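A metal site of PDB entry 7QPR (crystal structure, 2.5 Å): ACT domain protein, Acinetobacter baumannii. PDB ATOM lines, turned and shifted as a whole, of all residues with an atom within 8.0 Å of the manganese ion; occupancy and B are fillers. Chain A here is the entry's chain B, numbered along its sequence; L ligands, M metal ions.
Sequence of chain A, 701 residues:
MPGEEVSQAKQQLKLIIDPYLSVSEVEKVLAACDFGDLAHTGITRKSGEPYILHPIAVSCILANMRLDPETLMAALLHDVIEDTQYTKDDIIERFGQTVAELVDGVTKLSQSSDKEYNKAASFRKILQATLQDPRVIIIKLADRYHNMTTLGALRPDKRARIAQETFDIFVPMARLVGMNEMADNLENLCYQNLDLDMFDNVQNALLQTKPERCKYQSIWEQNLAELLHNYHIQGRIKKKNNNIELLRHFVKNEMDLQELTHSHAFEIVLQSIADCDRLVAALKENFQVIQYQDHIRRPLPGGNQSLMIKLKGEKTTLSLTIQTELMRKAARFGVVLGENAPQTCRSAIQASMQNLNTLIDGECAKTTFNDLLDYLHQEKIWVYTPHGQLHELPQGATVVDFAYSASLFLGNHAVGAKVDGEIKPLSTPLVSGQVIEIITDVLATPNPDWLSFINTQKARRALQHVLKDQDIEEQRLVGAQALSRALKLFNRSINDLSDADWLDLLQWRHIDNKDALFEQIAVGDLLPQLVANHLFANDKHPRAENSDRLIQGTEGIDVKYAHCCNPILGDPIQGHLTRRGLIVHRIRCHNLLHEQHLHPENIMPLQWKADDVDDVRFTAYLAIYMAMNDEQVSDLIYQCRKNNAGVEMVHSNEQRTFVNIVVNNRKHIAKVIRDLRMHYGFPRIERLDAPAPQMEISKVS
The side-chain carboxylate of Asp 143 is in salt-bridge range of the side-chain amino group of Lys 140, 3.2 Å away.
ND1 of His 54 sits at hydrogen-bond distance from NH1 of Arg 45 (3.3 Å).
The backbone carbonyl oxygen (O) of Ala 75 sits at hydrogen-bond distance from a ring nitrogen (ND1) of His 78, 2.8 Å away.
A ring nitrogen (ND1) of His 54 sits at hydrogen-bond distance from a ring nitrogen (ND1) of His 146, at 2.8 Å.
OD2 of Asp 79 sits close to OH of Tyr 51 (2.6 Å).
An oxygen (O16) of the ligand lies within salt-bridge range of the side-chain amino group (NZ) of Lys 140.
The guanidinium group (NH2) of Arg 144 lies within salt-bridge range of an oxygen (O16) of the ligand (3.2 Å).
O13 of the ligand lies within hydrogen-bond range of OG of Ser 110 (2.9 Å).
ND2 of Asn 147 sits at hydrogen-bond distance from O14 of the ligand (3.5 Å).
The backbone carbonyl oxygen (O) of Asn 147 is in hydrogen-bond range of a nitrogen (N4) of the ligand (2.9 Å).
The manganese ion is bound by the side-chain carboxylate (OD1) of Asp 143 (2.3 Å).
OD2 of Asp 79 is bound to the manganese ion (2.6 Å).
NE2 of His 54 binds the manganese ion, at 2.7 Å.
NE2 of His 78 binds the manganese ion (2.8 Å).
Residues that only touch the manganese ion: Tyr 51 (3.9 Å).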
ATOM      1  N   ARG A  45      32.889  -4.419  17.539  1.00  0.00           N
ATOM      2  CA  ARG A  45      31.704  -5.140  17.063  1.00  0.00           C
ATOM      3  C   ARG A  45      30.991  -5.888  18.223  1.00  0.00           C
ATOM      4  O   ARG A  45      31.489  -5.901  19.356  1.00  0.00           O
ATOM      5  CB  ARG A  45      32.116  -6.130  15.963  1.00  0.00           C
ATOM      6  CG  ARG A  45      32.890  -5.509  14.809  1.00  0.00           C
ATOM      7  CD  ARG A  45      32.047  -5.441  13.559  1.00  0.00           C
ATOM      8  NE  ARG A  45      31.735  -6.756  13.019  1.00  0.00           N
ATOM      9  CZ  ARG A  45      30.891  -6.997  12.009  1.00  0.00           C
ATOM     10  NH1 ARG A  45      30.262  -5.976  11.436  1.00  0.00           N
ATOM     11  NH2 ARG A  45      30.664  -8.213  11.582  1.00  0.00           N
ATOM     12  N   TYR A  51      36.137  -2.534  15.201  1.00  0.00           N
ATOM     13  CA  TYR A  51      35.202  -2.361  14.092  1.00  0.00           C
ATOM     14  C   TYR A  51      35.829  -2.437  12.708  1.00  0.00           C
ATOM     15  O   TYR A  51      35.294  -3.118  11.834  1.00  0.00           O
ATOM     16  CB  TYR A  51      34.359  -1.086  14.234  1.00  0.00           C
ATOM     17  CG  TYR A  51      33.108  -1.179  13.396  1.00  0.00           C
ATOM     18  CD1 TYR A  51      32.034  -1.975  13.800  1.00  0.00           C
ATOM     19  CD2 TYR A  51      33.023  -0.573  12.151  1.00  0.00           C
ATOM     20  CE1 TYR A  51      30.908  -2.131  13.001  1.00  0.00           C
ATOM     21  CE2 TYR A  51      31.902  -0.716  11.349  1.00  0.00           C
ATOM     22  CZ  TYR A  51      30.849  -1.500  11.777  1.00  0.00           C
ATOM     23  OH  TYR A  51      29.722  -1.646  10.999  1.00  0.00           O
ATOM     24  N   HIS A  54      35.877  -5.452  10.151  1.00  0.00           N
ATOM     25  CA  HIS A  54      34.774  -5.738   9.235  1.00  0.00           C
ATOM     26  C   HIS A  54      35.019  -5.061   7.871  1.00  0.00           C
ATOM     27  O   HIS A  54      35.205  -5.815   6.915  1.00  0.00           O
ATOM     28  CB  HIS A  54      33.395  -5.405   9.842  1.00  0.00           C
ATOM     29  CG  HIS A  54      32.267  -5.338   8.836  1.00  0.00           C
ATOM     30  ND1 HIS A  54      31.602  -6.478   8.430  1.00  0.00           N
ATOM     31  CD2 HIS A  54      31.738  -4.272   8.192  1.00  0.00           C
ATOM     32  CE1 HIS A  54      30.690  -6.071   7.552  1.00  0.00           C
ATOM     33  NE2 HIS A  54      30.746  -4.752   7.375  1.00  0.00           N
ATOM     34  N   PRO A  55      35.128  -3.711   7.724  1.00  0.00           N
ATOM     35  CA  PRO A  55      35.422  -3.153   6.396  1.00  0.00           C
ATOM     36  C   PRO A  55      36.704  -3.690   5.757  1.00  0.00           C
ATOM     37  O   PRO A  55      36.780  -3.752   4.526  1.00  0.00           O
ATOM     38  CB  PRO A  55      35.496  -1.645   6.658  1.00  0.00           C
ATOM     39  CG  PRO A  55      34.645  -1.440   7.842  1.00  0.00           C
ATOM     40  CD  PRO A  55      34.920  -2.635   8.706  1.00  0.00           C
ATOM     41  N   VAL A  58      35.777  -7.031   4.265  1.00  0.00           N
ATOM     42  CA  VAL A  58      34.928  -6.757   3.117  1.00  0.00           C
ATOM     43  C   VAL A  58      35.797  -6.356   1.936  1.00  0.00           C
ATOM     44  O   VAL A  58      35.627  -6.908   0.853  1.00  0.00           O
ATOM     45  CB  VAL A  58      33.851  -5.690   3.457  1.00  0.00           C
ATOM     46  CG1 VAL A  58      33.087  -5.255   2.215  1.00  0.00           C
ATOM     47  CG2 VAL A  58      32.897  -6.214   4.518  1.00  0.00           C
ATOM     48  N   ALA A  75      34.817   0.457   0.309  1.00  0.00           N
ATOM     49  CA  ALA A  75      34.508  -0.670   1.186  1.00  0.00           C
ATOM     50  C   ALA A  75      35.112  -0.462   2.560  1.00  0.00           C
ATOM     51  O   ALA A  75      34.492  -0.802   3.569  1.00  0.00           O
ATOM     52  CB  ALA A  75      35.026  -1.958   0.590  1.00  0.00           C
ATOM     53  N   HIS A  78      32.853   2.508   4.113  1.00  0.00           N
ATOM     54  CA  HIS A  78      31.408   2.545   3.905  1.00  0.00           C
ATOM     55  C   HIS A  78      30.582   2.804   5.161  1.00  0.00           C
ATOM     56  O   HIS A  78      29.468   3.295   5.056  1.00  0.00           O
ATOM     57  CB  HIS A  78      30.891   1.287   3.185  1.00  0.00           C
ATOM     58  CG  HIS A  78      30.753   0.073   4.046  1.00  0.00           C
ATOM     59  ND1 HIS A  78      31.853  -0.631   4.507  1.00  0.00           N
ATOM     60  CD2 HIS A  78      29.626  -0.557   4.463  1.00  0.00           C
ATOM     61  CE1 HIS A  78      31.372  -1.646   5.201  1.00  0.00           C
ATOM     62  NE2 HIS A  78      30.034  -1.650   5.202  1.00  0.00           N
ATOM     63  N   ASP A  79      31.138   2.495   6.330  1.00  0.00           N
ATOM     64  CA  ASP A  79      30.424   2.705   7.584  1.00  0.00           C
ATOM     65  C   ASP A  79      30.830   3.970   8.337  1.00  0.00           C
ATOM     66  O   ASP A  79      30.383   4.145   9.470  1.00  0.00           O
ATOM     67  CB  ASP A  79      30.590   1.498   8.518  1.00  0.00           C
ATOM     68  CG  ASP A  79      29.706   0.329   8.159  1.00  0.00           C
ATOM     69  OD1 ASP A  79      28.656   0.542   7.498  1.00  0.00           O
ATOM     70  OD2 ASP A  79      30.059  -0.814   8.542  1.00  0.00           O
ATOM     71  N   GLU A  82      27.680   6.980   8.522  1.00  0.00           N
ATOM     72  CA  GLU A  82      26.637   6.673   9.493  1.00  0.00           C
ATOM     73  C   GLU A  82      27.126   6.599  10.937  1.00  0.00           C
ATOM     74  O   GLU A  82      26.435   7.066  11.845  1.00  0.00           O
ATOM     75  CB  GLU A  82      25.935   5.343   9.098  1.00  0.00           C
ATOM     76  CG  GLU A  82      26.808   4.373   8.315  1.00  0.00           C
ATOM     77  CD  GLU A  82      26.092   3.291   7.526  1.00  0.00           C
ATOM     78  OE1 GLU A  82      24.899   3.045   7.809  1.00  0.00           O
ATOM     79  OE2 GLU A  82      26.736   2.698   6.627  1.00  0.00           O
ATOM     80  N   ASP A  83      28.310   6.022  11.161  1.00  0.00           N
ATOM     81  CA  ASP A  83      28.796   5.799  12.510  1.00  0.00           C
ATOM     82  C   ASP A  83      29.809   6.862  13.040  1.00  0.00           C
ATOM     83  O   ASP A  83      29.727   7.221  14.215  1.00  0.00           O
ATOM     84  CB  ASP A  83      29.381   4.380  12.640  1.00  0.00           C
ATOM     85  CG  ASP A  83      28.522   3.270  12.046  1.00  0.00           C
ATOM     86  OD1 ASP A  83      27.330   3.511  11.783  1.00  0.00           O
ATOM     87  OD2 ASP A  83      29.052   2.152  11.848  1.00  0.00           O
ATOM     88  N   VAL A 106      26.258   2.940  -1.044  1.00  0.00           N
ATOM     89  CA  VAL A 106      26.198   1.741  -0.201  1.00  0.00           C
ATOM     90  C   VAL A 106      25.415   2.011   1.080  1.00  0.00           C
ATOM     91  O   VAL A 106      24.609   1.190   1.501  1.00  0.00           O
ATOM     92  CB  VAL A 106      27.622   1.202   0.101  1.00  0.00           C
ATOM     93  CG1 VAL A 106      27.587   0.078   1.123  1.00  0.00           C
ATOM     94  CG2 VAL A 106      28.305   0.757  -1.178  1.00  0.00           C
ATOM     95  N   SER A 110      21.196   0.486   3.052  1.00  0.00           N
ATOM     96  CA  SER A 110      21.010  -0.115   4.355  1.00  0.00           C
ATOM     97  C   SER A 110      19.528  -0.223   4.723  1.00  0.00           C
ATOM     98  O   SER A 110      18.748   0.705   4.474  1.00  0.00           O
ATOM     99  CB  SER A 110      21.782   0.679   5.407  1.00  0.00           C
ATOM    100  OG  SER A 110      21.918  -0.033   6.623  1.00  0.00           O
ATOM    101  N   ILE A 139      29.861  -3.890  -3.459  1.00  0.00           N
ATOM    102  CA  ILE A 139      30.333  -3.592  -2.101  1.00  0.00           C
ATOM    103  C   ILE A 139      29.280  -4.039  -1.078  1.00  0.00           C
ATOM    104  O   ILE A 139      29.618  -4.647  -0.068  1.00  0.00           O
ATOM    105  CB  ILE A 139      30.642  -2.081  -1.919  1.00  0.00           C
ATOM    106  CG1 ILE A 139      31.718  -1.581  -2.885  1.00  0.00           C
ATOM    107  CG2 ILE A 139      30.998  -1.772  -0.461  1.00  0.00           C
ATOM    108  CD1 ILE A 139      31.819  -0.103  -2.942  1.00  0.00           C
ATOM    109  N   LYS A 140      28.005  -3.772  -1.367  1.00  0.00           N
ATOM    110  CA  LYS A 140      26.906  -4.145  -0.482  1.00  0.00           C
ATOM    111  C   LYS A 140      26.757  -5.649  -0.346  1.00  0.00           C
ATOM    112  O   LYS A 140      26.462  -6.126   0.737  1.00  0.00           O
ATOM    113  CB  LYS A 140      25.589  -3.474  -0.925  1.00  0.00           C
ATOM    114  CG  LYS A 140      24.421  -3.653   0.048  1.00  0.00           C
ATOM    115  CD  LYS A 140      24.755  -3.098   1.420  1.00  0.00           C
ATOM    116  CE  LYS A 140      23.685  -3.419   2.441  1.00  0.00           C
ATOM    117  NZ  LYS A 140      24.133  -3.078   3.817  1.00  0.00           N
ATOM    118  N   ALA A 142      29.269  -7.863  -0.656  1.00  0.00           N
ATOM    119  CA  ALA A 142      30.433  -8.293   0.111  1.00  0.00           C
ATOM    120  C   ALA A 142      30.230  -7.946   1.599  1.00  0.00           C
ATOM    121  O   ALA A 142      30.537  -8.757   2.481  1.00  0.00           O
ATOM    122  CB  ALA A 142      31.693  -7.620  -0.427  1.00  0.00           C
ATOM    123  N   ASP A 143      29.640  -6.768   1.868  1.00  0.00           N
ATOM    124  CA  ASP A 143      29.329  -6.310   3.217  1.00  0.00           C
ATOM    125  C   ASP A 143      28.302  -7.275   3.836  1.00  0.00           C
ATOM    126  O   ASP A 143      28.530  -7.770   4.940  1.00  0.00           O
ATOM    127  CB  ASP A 143      28.775  -4.873   3.195  1.00  0.00           C
ATOM    128  CG  ASP A 143      28.084  -4.447   4.469  1.00  0.00           C
ATOM    129  OD1 ASP A 143      28.789  -4.051   5.424  1.00  0.00           O
ATOM    130  OD2 ASP A 143      26.830  -4.550   4.527  1.00  0.00           O
ATOM    131  N   ARG A 144      27.204  -7.551   3.122  1.00  0.00           N
ATOM    132  CA  ARG A 144      26.185  -8.453   3.613  1.00  0.00           C
ATOM    133  C   ARG A 144      26.744  -9.850   3.835  1.00  0.00           C
ATOM    134  O   ARG A 144      26.435 -10.461   4.848  1.00  0.00           O
ATOM    135  CB  ARG A 144      24.949  -8.494   2.703  1.00  0.00           C
ATOM    136  CG  ARG A 144      23.855  -9.462   3.171  1.00  0.00           C
ATOM    137  CD  ARG A 144      23.353  -9.163   4.581  1.00  0.00           C
ATOM    138  NE  ARG A 144      22.806  -7.809   4.685  1.00  0.00           N
ATOM    139  CZ  ARG A 144      21.537  -7.523   4.437  1.00  0.00           C
ATOM    140  NH1 ARG A 144      20.663  -8.439   4.078  1.00  0.00           N
ATOM    141  NH2 ARG A 144      21.128  -6.241   4.548  1.00  0.00           N
ATOM    142  N   HIS A 146      29.890 -10.705   4.700  1.00  0.00           N
ATOM    143  CA  HIS A 146      30.681 -10.721   5.923  1.00  0.00           C
ATOM    144  C   HIS A 146      29.788 -10.706   7.156  1.00  0.00           C
ATOM    145  O   HIS A 146      30.074 -11.405   8.139  1.00  0.00           O
ATOM    146  CB  HIS A 146      31.688  -9.580   5.948  1.00  0.00           C
ATOM    147  CG  HIS A 146      32.702  -9.755   7.024  1.00  0.00           C
ATOM    148  ND1 HIS A 146      32.627  -9.042   8.202  1.00  0.00           N
ATOM    149  CD2 HIS A 146      33.753 -10.615   7.095  1.00  0.00           C
ATOM    150  CE1 HIS A 146      33.636  -9.464   8.948  1.00  0.00           C
ATOM    151  NE2 HIS A 146      34.344 -10.408   8.312  1.00  0.00           N
ATOM    152  N   ASN A 147      28.694  -9.935   7.098  1.00  0.00           N
ATOM    153  CA  ASN A 147      27.716  -9.856   8.181  1.00  0.00           C
ATOM    154  C   ASN A 147      27.040 -11.213   8.399  1.00  0.00           C
ATOM    155  O   ASN A 147      26.852 -11.597   9.555  1.00  0.00           O
ATOM    156  CB  ASN A 147      26.654  -8.810   7.885  1.00  0.00           C
ATOM    157  CG  ASN A 147      27.089  -7.401   8.217  1.00  0.00           C
ATOM    158  OD1 ASN A 147      27.919  -7.186   9.114  1.00  0.00           O
ATOM    159  ND2 ASN A 147      26.540  -6.429   7.495  1.00  0.00           N
HETATM  160  P1  LIG L   1      20.692  -3.087  15.482  1.00  0.00           P
HETATM  161  O1  LIG L   1      21.148  -1.683  15.773  1.00  0.00           O
HETATM  162  O2  LIG L   1      21.816  -4.079  15.325  1.00  0.00           O
HETATM  163  O3  LIG L   1      19.578  -3.560  16.376  1.00  0.00           O
HETATM  164  O4  LIG L   1      19.996  -3.013  14.044  1.00  0.00           O
HETATM  165  P2  LIG L   1      20.562  -2.129  12.826  1.00  0.00           P
HETATM  166  O5  LIG L   1      20.011  -2.701  11.537  1.00  0.00           O
HETATM  167  O6  LIG L   1      20.334  -0.672  13.148  1.00  0.00           O
HETATM  168  O7  LIG L   1      22.142  -2.426  12.861  1.00  0.00           O
HETATM  169  C1  LIG L   1      22.705  -3.551  12.182  1.00  0.00           C
HETATM  170  C2  LIG L   1      24.194  -3.314  12.061  1.00  0.00           C
HETATM  171  O8  LIG L   1      24.919  -4.048  13.057  1.00  0.00           O
HETATM  172  C3  LIG L   1      24.760  -3.777  10.731  1.00  0.00           C
HETATM  173  O9  LIG L   1      24.916  -2.654   9.863  1.00  0.00           O
HETATM  174  C4  LIG L   1      26.076  -4.453  11.081  1.00  0.00           C
HETATM  175  O10 LIG L   1      27.174  -3.950  10.313  1.00  0.00           O
HETATM  176  C5  LIG L   1      26.253  -4.168  12.568  1.00  0.00           C
HETATM  177  N1  LIG L   1      27.037  -5.204  13.324  1.00  0.00           N
HETATM  178  C6  LIG L   1      27.858  -4.880  14.334  1.00  0.00           C
HETATM  179  N2  LIG L   1      28.455  -5.962  14.868  1.00  0.00           N
HETATM  180  C7  LIG L   1      28.013  -7.022  14.186  1.00  0.00           C
HETATM  181  C8  LIG L   1      28.257  -8.480  14.240  1.00  0.00           C
HETATM  182  O11 LIG L   1      29.043  -8.969  15.079  1.00  0.00           O
HETATM  183  N3  LIG L   1      27.623  -9.247  13.365  1.00  0.00           N
HETATM  184  C9  LIG L   1      26.782  -8.749  12.452  1.00  0.00           C
HETATM  185  N4  LIG L   1      26.176  -9.598  11.603  1.00  0.00           N
HETATM  186  N5  LIG L   1      26.505  -7.423  12.340  1.00  0.00           N
HETATM  187  C10 LIG L   1      27.082  -6.521  13.163  1.00  0.00           C
HETATM  188  P3  LIG L   1      24.178  -2.586   8.442  1.00  0.00           P
HETATM  189  O12 LIG L   1      25.149  -1.999   7.447  1.00  0.00           O
HETATM  190  O13 LIG L   1      22.837  -1.943   8.632  1.00  0.00           O
HETATM  191  O14 LIG L   1      23.978  -4.137   8.082  1.00  0.00           O
HETATM  192  P4  LIG L   1      22.521  -4.790   7.895  1.00  0.00           P
HETATM  193  O15 LIG L   1      22.849  -6.240   7.665  1.00  0.00           O
HETATM  194  O16 LIG L   1      21.948  -4.061   6.702  1.00  0.00           O
HETATM  195  O17 LIG L   1      21.791  -4.560   9.188  1.00  0.00           O
HETATM  196 MN    MN M   1      28.860  -2.847   7.440  1.00  0.00          MN
